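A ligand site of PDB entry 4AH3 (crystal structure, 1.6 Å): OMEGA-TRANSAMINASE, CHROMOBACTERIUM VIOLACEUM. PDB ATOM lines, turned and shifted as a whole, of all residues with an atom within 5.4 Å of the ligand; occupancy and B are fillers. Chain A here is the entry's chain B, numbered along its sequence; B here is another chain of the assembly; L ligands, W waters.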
ATOM      1  N   SER A 119      27.895  -9.613  14.061  1.00  0.00           N
ATOM      2  CA  SER A 119      28.035  -8.218  14.454  1.00  0.00           C
ATOM      3  C   SER A 119      27.664  -7.314  13.271  1.00  0.00           C
ATOM      4  O   SER A 119      27.643  -7.758  12.133  1.00  0.00           O
ATOM      5  CB  SER A 119      29.471  -7.891  14.845  1.00  0.00           C
ATOM      6  OG  SER A 119      30.342  -8.040  13.712  1.00  0.00           O
ATOM      7  N   GLY A 120      27.410  -6.040  13.545  1.00  0.00           N
ATOM      8  CA  GLY A 120      27.210  -5.069  12.465  1.00  0.00           C
ATOM      9  C   GLY A 120      28.442  -4.926  11.588  1.00  0.00           C
ATOM     10  O   GLY A 120      28.325  -4.711  10.382  1.00  0.00           O
ATOM     11  N   SER A 121      29.619  -5.065  12.189  1.00  0.00           N
ATOM     12  CA  SER A 121      30.871  -4.893  11.483  1.00  0.00           C
ATOM     13  C   SER A 121      31.077  -6.026  10.503  1.00  0.00           C
ATOM     14  O   SER A 121      31.456  -5.805   9.327  1.00  0.00           O
ATOM     15  CB  SER A 121      32.037  -4.810  12.455  1.00  0.00           C
ATOM     16  OG  SER A 121      31.954  -3.611  13.231  1.00  0.00           O
ATOM     17  N   GLU A 122      30.839  -7.252  10.961  1.00  0.00           N
ATOM     18  CA  GLU A 122      30.893  -8.372  10.045  1.00  0.00           C
ATOM     19  C   GLU A 122      29.845  -8.211   8.935  1.00  0.00           C
ATOM     20  O   GLU A 122      30.113  -8.589   7.793  1.00  0.00           O
ATOM     21  CB  GLU A 122      30.704  -9.698  10.796  1.00  0.00           C
ATOM     22  CG  GLU A 122      31.891 -10.219  11.591  1.00  0.00           C
ATOM     23  CD  GLU A 122      31.487 -11.444  12.407  1.00  0.00           C
ATOM     24  OE1 GLU A 122      30.399 -12.008  12.146  1.00  0.00           O
ATOM     25  OE2 GLU A 122      32.228 -11.839  13.314  1.00  0.00           O
ATOM     26  N   VAL A 124      28.777  -5.443   7.561  1.00  0.00           N
ATOM     27  CA  VAL A 124      29.329  -4.504   6.604  1.00  0.00           C
ATOM     28  C   VAL A 124      30.400  -5.173   5.736  1.00  0.00           C
ATOM     29  O   VAL A 124      30.385  -4.986   4.517  1.00  0.00           O
ATOM     30  CB  VAL A 124      29.880  -3.238   7.304  1.00  0.00           C
ATOM     31  CG1 VAL A 124      30.598  -2.312   6.325  1.00  0.00           C
ATOM     32  CG2 VAL A 124      28.769  -2.428   7.973  1.00  0.00           C
ATOM     33  N   TYR A 153      29.746   5.992   9.862  1.00  0.00           N
ATOM     34  CA  TYR A 153      30.302   4.922  10.655  1.00  0.00           C
ATOM     35  C   TYR A 153      29.701   3.608  10.199  1.00  0.00           C
ATOM     36  O   TYR A 153      28.488   3.450  10.142  1.00  0.00           O
ATOM     37  CB  TYR A 153      29.983   5.097  12.157  1.00  0.00           C
ATOM     38  CG  TYR A 153      30.700   4.053  12.982  1.00  0.00           C
ATOM     39  CD1 TYR A 153      32.050   4.198  13.265  1.00  0.00           C
ATOM     40  CD2 TYR A 153      30.049   2.918  13.463  1.00  0.00           C
ATOM     41  CE1 TYR A 153      32.746   3.237  14.008  1.00  0.00           C
ATOM     42  CE2 TYR A 153      30.723   1.960  14.218  1.00  0.00           C
ATOM     43  CZ  TYR A 153      32.066   2.124  14.492  1.00  0.00           C
ATOM     44  OH  TYR A 153      32.725   1.167  15.228  1.00  0.00           O
ATOM     45  N   HIS A 154      30.588   2.669   9.845  1.00  0.00           N
ATOM     46  CA  HIS A 154      30.169   1.357   9.300  1.00  0.00           C
ATOM     47  C   HIS A 154      30.932   0.235   9.929  1.00  0.00           C
ATOM     48  O   HIS A 154      31.164  -0.832   9.341  1.00  0.00           O
ATOM     49  CB  HIS A 154      30.308   1.349   7.766  1.00  0.00           C
ATOM     50  CG  HIS A 154      29.455   2.390   7.110  1.00  0.00           C
ATOM     51  ND1 HIS A 154      28.133   2.338   7.141  1.00  0.00           N
ATOM     52  CD2 HIS A 154      29.787   3.600   6.482  1.00  0.00           C
ATOM     53  CE1 HIS A 154      27.630   3.423   6.516  1.00  0.00           C
ATOM     54  NE2 HIS A 154      28.648   4.206   6.151  1.00  0.00           N
ATOM     55  N   GLY A 155      31.338   0.466  11.172  1.00  0.00           N
ATOM     56  CA  GLY A 155      31.897  -0.607  11.980  1.00  0.00           C
ATOM     57  C   GLY A 155      33.386  -0.513  12.114  1.00  0.00           C
ATOM     58  O   GLY A 155      34.015   0.470  11.738  1.00  0.00           O
ATOM     59  N   SER A 156      33.950  -1.615  12.612  1.00  0.00           N
ATOM     60  CA  SER A 156      35.297  -1.652  13.088  1.00  0.00           C
ATOM     61  C   SER A 156      36.188  -2.724  12.493  1.00  0.00           C
ATOM     62  O   SER A 156      37.334  -2.857  12.918  1.00  0.00           O
ATOM     63  CB  SER A 156      35.310  -1.799  14.602  1.00  0.00           C
ATOM     64  OG  SER A 156      36.569  -1.412  15.042  1.00  0.00           O
ATOM     65  N   GLU A 226      24.240   5.309   6.371  1.00  0.00           N
ATOM     66  CA  GLU A 226      23.288   5.256   7.451  1.00  0.00           C
ATOM     67  C   GLU A 226      22.133   6.215   7.128  1.00  0.00           C
ATOM     68  O   GLU A 226      22.367   7.352   6.765  1.00  0.00           O
ATOM     69  CB  GLU A 226      23.991   5.725   8.709  1.00  0.00           C
ATOM     70  CG  GLU A 226      25.166   4.910   9.167  1.00  0.00           C
ATOM     71  CD  GLU A 226      25.996   5.749  10.105  1.00  0.00           C
ATOM     72  OE1 GLU A 226      26.828   6.527   9.647  1.00  0.00           O
ATOM     73  OE2 GLU A 226      25.702   5.638  11.308  1.00  0.00           O
ATOM     74  N   ALA A 231      26.764   7.272  15.084  1.00  0.00           N
ATOM     75  CA  ALA A 231      28.016   7.643  15.743  1.00  0.00           C
ATOM     76  C   ALA A 231      28.560   9.031  15.431  1.00  0.00           C
ATOM     77  O   ALA A 231      29.287   9.574  16.243  1.00  0.00           O
ATOM     78  CB  ALA A 231      29.085   6.572  15.480  1.00  0.00           C
ATOM     79  N   ASP A 259      22.834   1.335   5.730  1.00  0.00           N
ATOM     80  CA  ASP A 259      23.376   0.716   6.912  1.00  0.00           C
ATOM     81  C   ASP A 259      22.369   0.945   8.039  1.00  0.00           C
ATOM     82  O   ASP A 259      22.260   2.045   8.616  1.00  0.00           O
ATOM     83  CB  ASP A 259      24.744   1.224   7.273  1.00  0.00           C
ATOM     84  CG  ASP A 259      25.359   0.473   8.450  1.00  0.00           C
ATOM     85  OD1 ASP A 259      24.646  -0.305   9.135  1.00  0.00           O
ATOM     86  OD2 ASP A 259      26.561   0.647   8.668  1.00  0.00           O
ATOM     87  N   VAL A 261      22.156  -0.586  10.934  1.00  0.00           N
ATOM     88  CA  VAL A 261      22.565  -1.232  12.190  1.00  0.00           C
ATOM     89  C   VAL A 261      21.961  -0.430  13.355  1.00  0.00           C
ATOM     90  O   VAL A 261      21.433  -1.058  14.282  1.00  0.00           O
ATOM     91  CB  VAL A 261      24.073  -1.443  12.303  1.00  0.00           C
ATOM     92  CG1 VAL A 261      24.433  -1.903  13.695  1.00  0.00           C
ATOM     93  CG2 VAL A 261      24.507  -2.524  11.308  1.00  0.00           C
ATOM     94  N   ILE A 262      21.995   0.900  13.286  1.00  0.00           N
ATOM     95  CA  ILE A 262      21.288   1.685  14.329  1.00  0.00           C
ATOM     96  C   ILE A 262      19.798   1.901  14.052  1.00  0.00           C
ATOM     97  O   ILE A 262      18.915   1.690  14.939  1.00  0.00           O
ATOM     98  CB  ILE A 262      21.957   3.054  14.628  1.00  0.00           C
ATOM     99  CG1 ILE A 262      23.249   2.819  15.392  1.00  0.00           C
ATOM    100  CG2 ILE A 262      21.001   3.953  15.408  1.00  0.00           C
ATOM    101  CD1 ILE A 262      24.048   4.060  15.733  1.00  0.00           C
ATOM    102  N   ALA A 287      22.039  -5.240  12.793  1.00  0.00           N
ATOM    103  CA  ALA A 287      22.522  -5.903  14.009  1.00  0.00           C
ATOM    104  C   ALA A 287      21.829  -5.183  15.147  1.00  0.00           C
ATOM    105  O   ALA A 287      20.643  -4.855  15.042  1.00  0.00           O
ATOM    106  CB  ALA A 287      24.031  -5.799  14.126  1.00  0.00           C
ATOM    107  N   LYS A 288      22.561  -4.907  16.228  1.00  0.00           N
ATOM    108  CA  LYS A 288      22.008  -4.080  17.328  1.00  0.00           C
ATOM    109  C   LYS A 288      20.594  -4.532  17.740  1.00  0.00           C
ATOM    110  O   LYS A 288      20.413  -5.569  18.371  1.00  0.00           O
ATOM    111  CB  LYS A 288      22.193  -2.575  16.953  1.00  0.00           C
ATOM    112  CG  LYS A 288      23.619  -2.085  17.254  1.00  0.00           C
ATOM    113  CD  LYS A 288      23.954  -0.589  17.030  1.00  0.00           C
ATOM    114  CE  LYS A 288      25.447  -0.211  17.272  1.00  0.00           C
ATOM    115  NZ  LYS A 288      26.174   0.372  16.118  1.00  0.00           N
ATOM    116  N   PHE B  88      32.393   0.496  25.842  1.00  0.00           N
ATOM    117  CA  PHE B  88      32.865   1.691  25.101  1.00  0.00           C
ATOM    118  C   PHE B  88      32.856   2.968  25.965  1.00  0.00           C
ATOM    119  O   PHE B  88      33.589   3.930  25.689  1.00  0.00           O
ATOM    120  CB  PHE B  88      31.912   2.008  23.928  1.00  0.00           C
ATOM    121  CG  PHE B  88      31.995   1.067  22.741  1.00  0.00           C
ATOM    122  CD1 PHE B  88      31.729  -0.289  22.861  1.00  0.00           C
ATOM    123  CD2 PHE B  88      32.223   1.599  21.468  1.00  0.00           C
ATOM    124  CE1 PHE B  88      31.777  -1.104  21.744  1.00  0.00           C
ATOM    125  CE2 PHE B  88      32.275   0.768  20.346  1.00  0.00           C
ATOM    126  CZ  PHE B  88      32.035  -0.583  20.477  1.00  0.00           C
ATOM    127  N   GLU B 122      36.904 -11.644  13.404  1.00  0.00           N
ATOM    128  CA  GLU B 122      37.042 -10.318  13.989  1.00  0.00           C
ATOM    129  C   GLU B 122      38.314 -10.248  14.819  1.00  0.00           C
ATOM    130  O   GLU B 122      38.953  -9.215  14.901  1.00  0.00           O
ATOM    131  CB  GLU B 122      35.860  -9.995  14.892  1.00  0.00           C
ATOM    132  CG  GLU B 122      34.572  -9.552  14.213  1.00  0.00           C
ATOM    133  CD  GLU B 122      33.453  -9.371  15.235  1.00  0.00           C
ATOM    134  OE1 GLU B 122      33.756  -9.464  16.442  1.00  0.00           O
ATOM    135  OE2 GLU B 122      32.286  -9.161  14.867  1.00  0.00           O
ATOM    136  N   GLY B 319      36.697  -1.621  17.816  1.00  0.00           N
ATOM    137  CA  GLY B 319      35.876  -2.400  18.715  1.00  0.00           C
ATOM    138  C   GLY B 319      34.496  -2.665  18.192  1.00  0.00           C
ATOM    139  O   GLY B 319      34.048  -2.026  17.229  1.00  0.00           O
ATOM    140  N   PHE B 320      33.806  -3.598  18.833  1.00  0.00           N
ATOM    141  CA  PHE B 320      32.478  -3.981  18.371  1.00  0.00           C
ATOM    142  C   PHE B 320      31.418  -3.823  19.450  1.00  0.00           C
ATOM    143  O   PHE B 320      31.692  -4.020  20.642  1.00  0.00           O
ATOM    144  CB  PHE B 320      32.502  -5.422  17.839  1.00  0.00           C
ATOM    145  CG  PHE B 320      33.669  -5.694  16.913  1.00  0.00           C
ATOM    146  CD1 PHE B 320      33.562  -5.431  15.560  1.00  0.00           C
ATOM    147  CD2 PHE B 320      34.872  -6.178  17.417  1.00  0.00           C
ATOM    148  CE1 PHE B 320      34.639  -5.662  14.706  1.00  0.00           C
ATOM    149  CE2 PHE B 320      35.957  -6.404  16.577  1.00  0.00           C
ATOM    150  CZ  PHE B 320      35.831  -6.151  15.218  1.00  0.00           C
ATOM    151  N   THR B 321      30.192  -3.465  19.043  1.00  0.00           N
ATOM    152  CA  THR B 321      29.084  -3.290  20.003  1.00  0.00           C
ATOM    153  C   THR B 321      29.067  -4.419  21.045  1.00  0.00           C
ATOM    154  O   THR B 321      29.007  -4.144  22.292  1.00  0.00           O
ATOM    155  CB  THR B 321      27.721  -3.204  19.253  1.00  0.00           C
ATOM    156  OG1 THR B 321      27.738  -2.032  18.426  1.00  0.00           O
ATOM    157  CG2 THR B 321      26.497  -3.128  20.181  1.00  0.00           C
ATOM    158  N   TYR B 322      29.102  -5.654  20.545  1.00  0.00           N
ATOM    159  CA  TYR B 322      29.019  -6.827  21.423  1.00  0.00           C
ATOM    160  C   TYR B 322      30.329  -7.358  21.991  1.00  0.00           C
ATOM    161  O   TYR B 322      30.342  -8.466  22.537  1.00  0.00           O
ATOM    162  CB  TYR B 322      28.231  -7.976  20.796  1.00  0.00           C
ATOM    163  CG  TYR B 322      26.874  -7.551  20.320  1.00  0.00           C
ATOM    164  CD1 TYR B 322      26.049  -6.780  21.142  1.00  0.00           C
ATOM    165  CD2 TYR B 322      26.396  -7.928  19.055  1.00  0.00           C
ATOM    166  CE1 TYR B 322      24.804  -6.381  20.725  1.00  0.00           C
ATOM    167  CE2 TYR B 322      25.155  -7.532  18.629  1.00  0.00           C
ATOM    168  CZ  TYR B 322      24.363  -6.761  19.467  1.00  0.00           C
ATOM    169  OH  TYR B 322      23.124  -6.368  19.077  1.00  0.00           O
HETATM  170  N1  LIG L   1      27.112   0.256  11.257  1.00  0.00           N
HETATM  171  C1  LIG L   1      26.534   1.205  12.034  1.00  0.00           C
HETATM  172  C2  LIG L   1      25.673   2.275  11.445  1.00  0.00           C
HETATM  173  C3  LIG L   1      26.693   1.176  13.498  1.00  0.00           C
HETATM  174  O1  LIG L   1      26.081   2.114  14.228  1.00  0.00           O
HETATM  175  C4  LIG L   1      27.514   0.159  14.144  1.00  0.00           C
HETATM  176  C5  LIG L   1      27.580   0.175  15.665  1.00  0.00           C
HETATM  177  C6  LIG L   1      28.100  -0.827  13.188  1.00  0.00           C
HETATM  178  C7  LIG L   1      27.897  -0.703  11.812  1.00  0.00           C
HETATM  179  C8  LIG L   1      28.985  -1.948  13.645  1.00  0.00           C
HETATM  180  O2  LIG L   1      28.227  -2.873  14.434  1.00  0.00           O
HETATM  181  P1  LIG L   1      29.054  -3.759  15.510  1.00  0.00           P
HETATM  182  O3  LIG L   1      30.185  -4.467  14.784  1.00  0.00           O
HETATM  183  O4  LIG L   1      29.608  -2.865  16.614  1.00  0.00           O
HETATM  184  O5  LIG L   1      28.035  -4.697  15.991  1.00  0.00           O
HETATM  185  O   HOH W   1      26.914   4.831  13.712  1.00  0.00           O
HETATM  186  O   HOH W   2      31.604  -1.144  15.910  1.00  0.00           O
HETATM  187  O   HOH W   3      28.949  -6.457  17.940  1.00  0.00           O
HETATM  188  O   HOH W   4      25.353  -4.874  16.997  1.00  0.00           O
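The side-chain hydroxyl of Thr 321 of chain B sits at hydrogen-bond distance from an oxygen (O4) of the ligand, at 2.7 Å. The side-chain carboxylate (OD2) of Asp 259 lies within hydrogen-bond range of a nitrogen (N1) of the ligand, 2.7 Å away. The side-chain amino group of Lys 288 is bonded to a carbon (C5) of the ligand, at 1.5 Å. N of Gly 120 sits at hydrogen-bond distance from O5 of the ligand (2.9 Å). The side-chain hydroxyl (OG) of Ser 121 sits at hydrogen-bond distance from an oxygen (O3) of the ligand (2.5 Å). The backbone NH (N) of Thr 321 of chain B lies within hydrogen-bond range of an oxygen (O4) of the ligand, at 2.6 Å. N of Ser 121 lies within hydrogen-bond range of O3 of the ligand (2.7 Å).
The side-chain carboxylate of Asp 259 sits at hydrogen-bond distance from the backbone NH of Val 261, at 3.1 Å. The backbone NH of Tyr 153 lies within hydrogen-bond range of the side-chain carboxylate of Glu 226 (3.0 Å). OG of Ser 121 is in hydrogen-bond range of N of Ser 156 (2.9 Å). The side-chain carboxylate (OE2) of Glu 122 of chain B sits at hydrogen-bond distance from the side-chain hydroxyl (OG) of Ser 119 (2.5 Å). The backbone NH (N) of Ser 121 sits close to the side-chain hydroxyl (OG) of Ser 119. The side-chain hydroxyl (OG) of Ser 119 sits at hydrogen-bond distance from the backbone NH (N) of Glu 122 of chain A. O of Lys 288 sits at hydrogen-bond distance from OH of Tyr 322 of chain B (2.9 Å). The side-chain carboxylate (OD2) of Asp 259 lies within hydrogen-bond range of a ring nitrogen (ND1) of His 154 (2.8 Å).
Ser 119 touches the ligand. Tyr 153 touches the ligand (O to C2, 3.3 Å). His 154 touches the ligand (C to C7, 3.7 Å). Gly 155 touches the ligand (CA to C8, 3.6 Å). Glu 226 touches the ligand. Val 261 touches the ligand. Ile 262 touches the ligand. C of Phe 320 of chain B touches O4 of the ligand, 3.5 Å away. Hydrophobic or aromatic side chains that line the ligand: Tyr 153, Val 261, Ile 262 and Phe 320 of chain B. Of the 22 residues printed, 13 come within 4 Å of the ligand. The nearest printed residue that does not touch the ligand is Val 124 (4.3 Å).
Water W2 lies within hydrogen-bond range of the side-chain hydroxyl (OH) of Tyr 153 (2.7 Å), an oxygen (O4) of the ligand (2.7 Å) and the backbone carbonyl oxygen (O) of Gly 319 of chain B (2.9 Å). Water W3 lies within hydrogen-bond range of the backbone NH (N) of Tyr 322 of chain B (2.7 Å), an oxygen (O5) of the ligand (2.8 Å) and the backbone NH (N) of Thr 321 of chain B (3.4 Å). Water W4 lies within hydrogen-bond range of an oxygen (O5) of the ligand (2.9 Å), the backbone NH (N) of Lys 288 (2.9 Å) and the side-chain hydroxyl (OH) of Tyr 322 of chain B (3.4 Å). Water W1 lies within hydrogen-bond range of the backbone NH (N) of Ala 231 (2.8 Å), the side-chain carboxylate (OE2) of Glu 226 (2.8 Å) and an oxygen (O1) of the ligand (2.9 Å).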
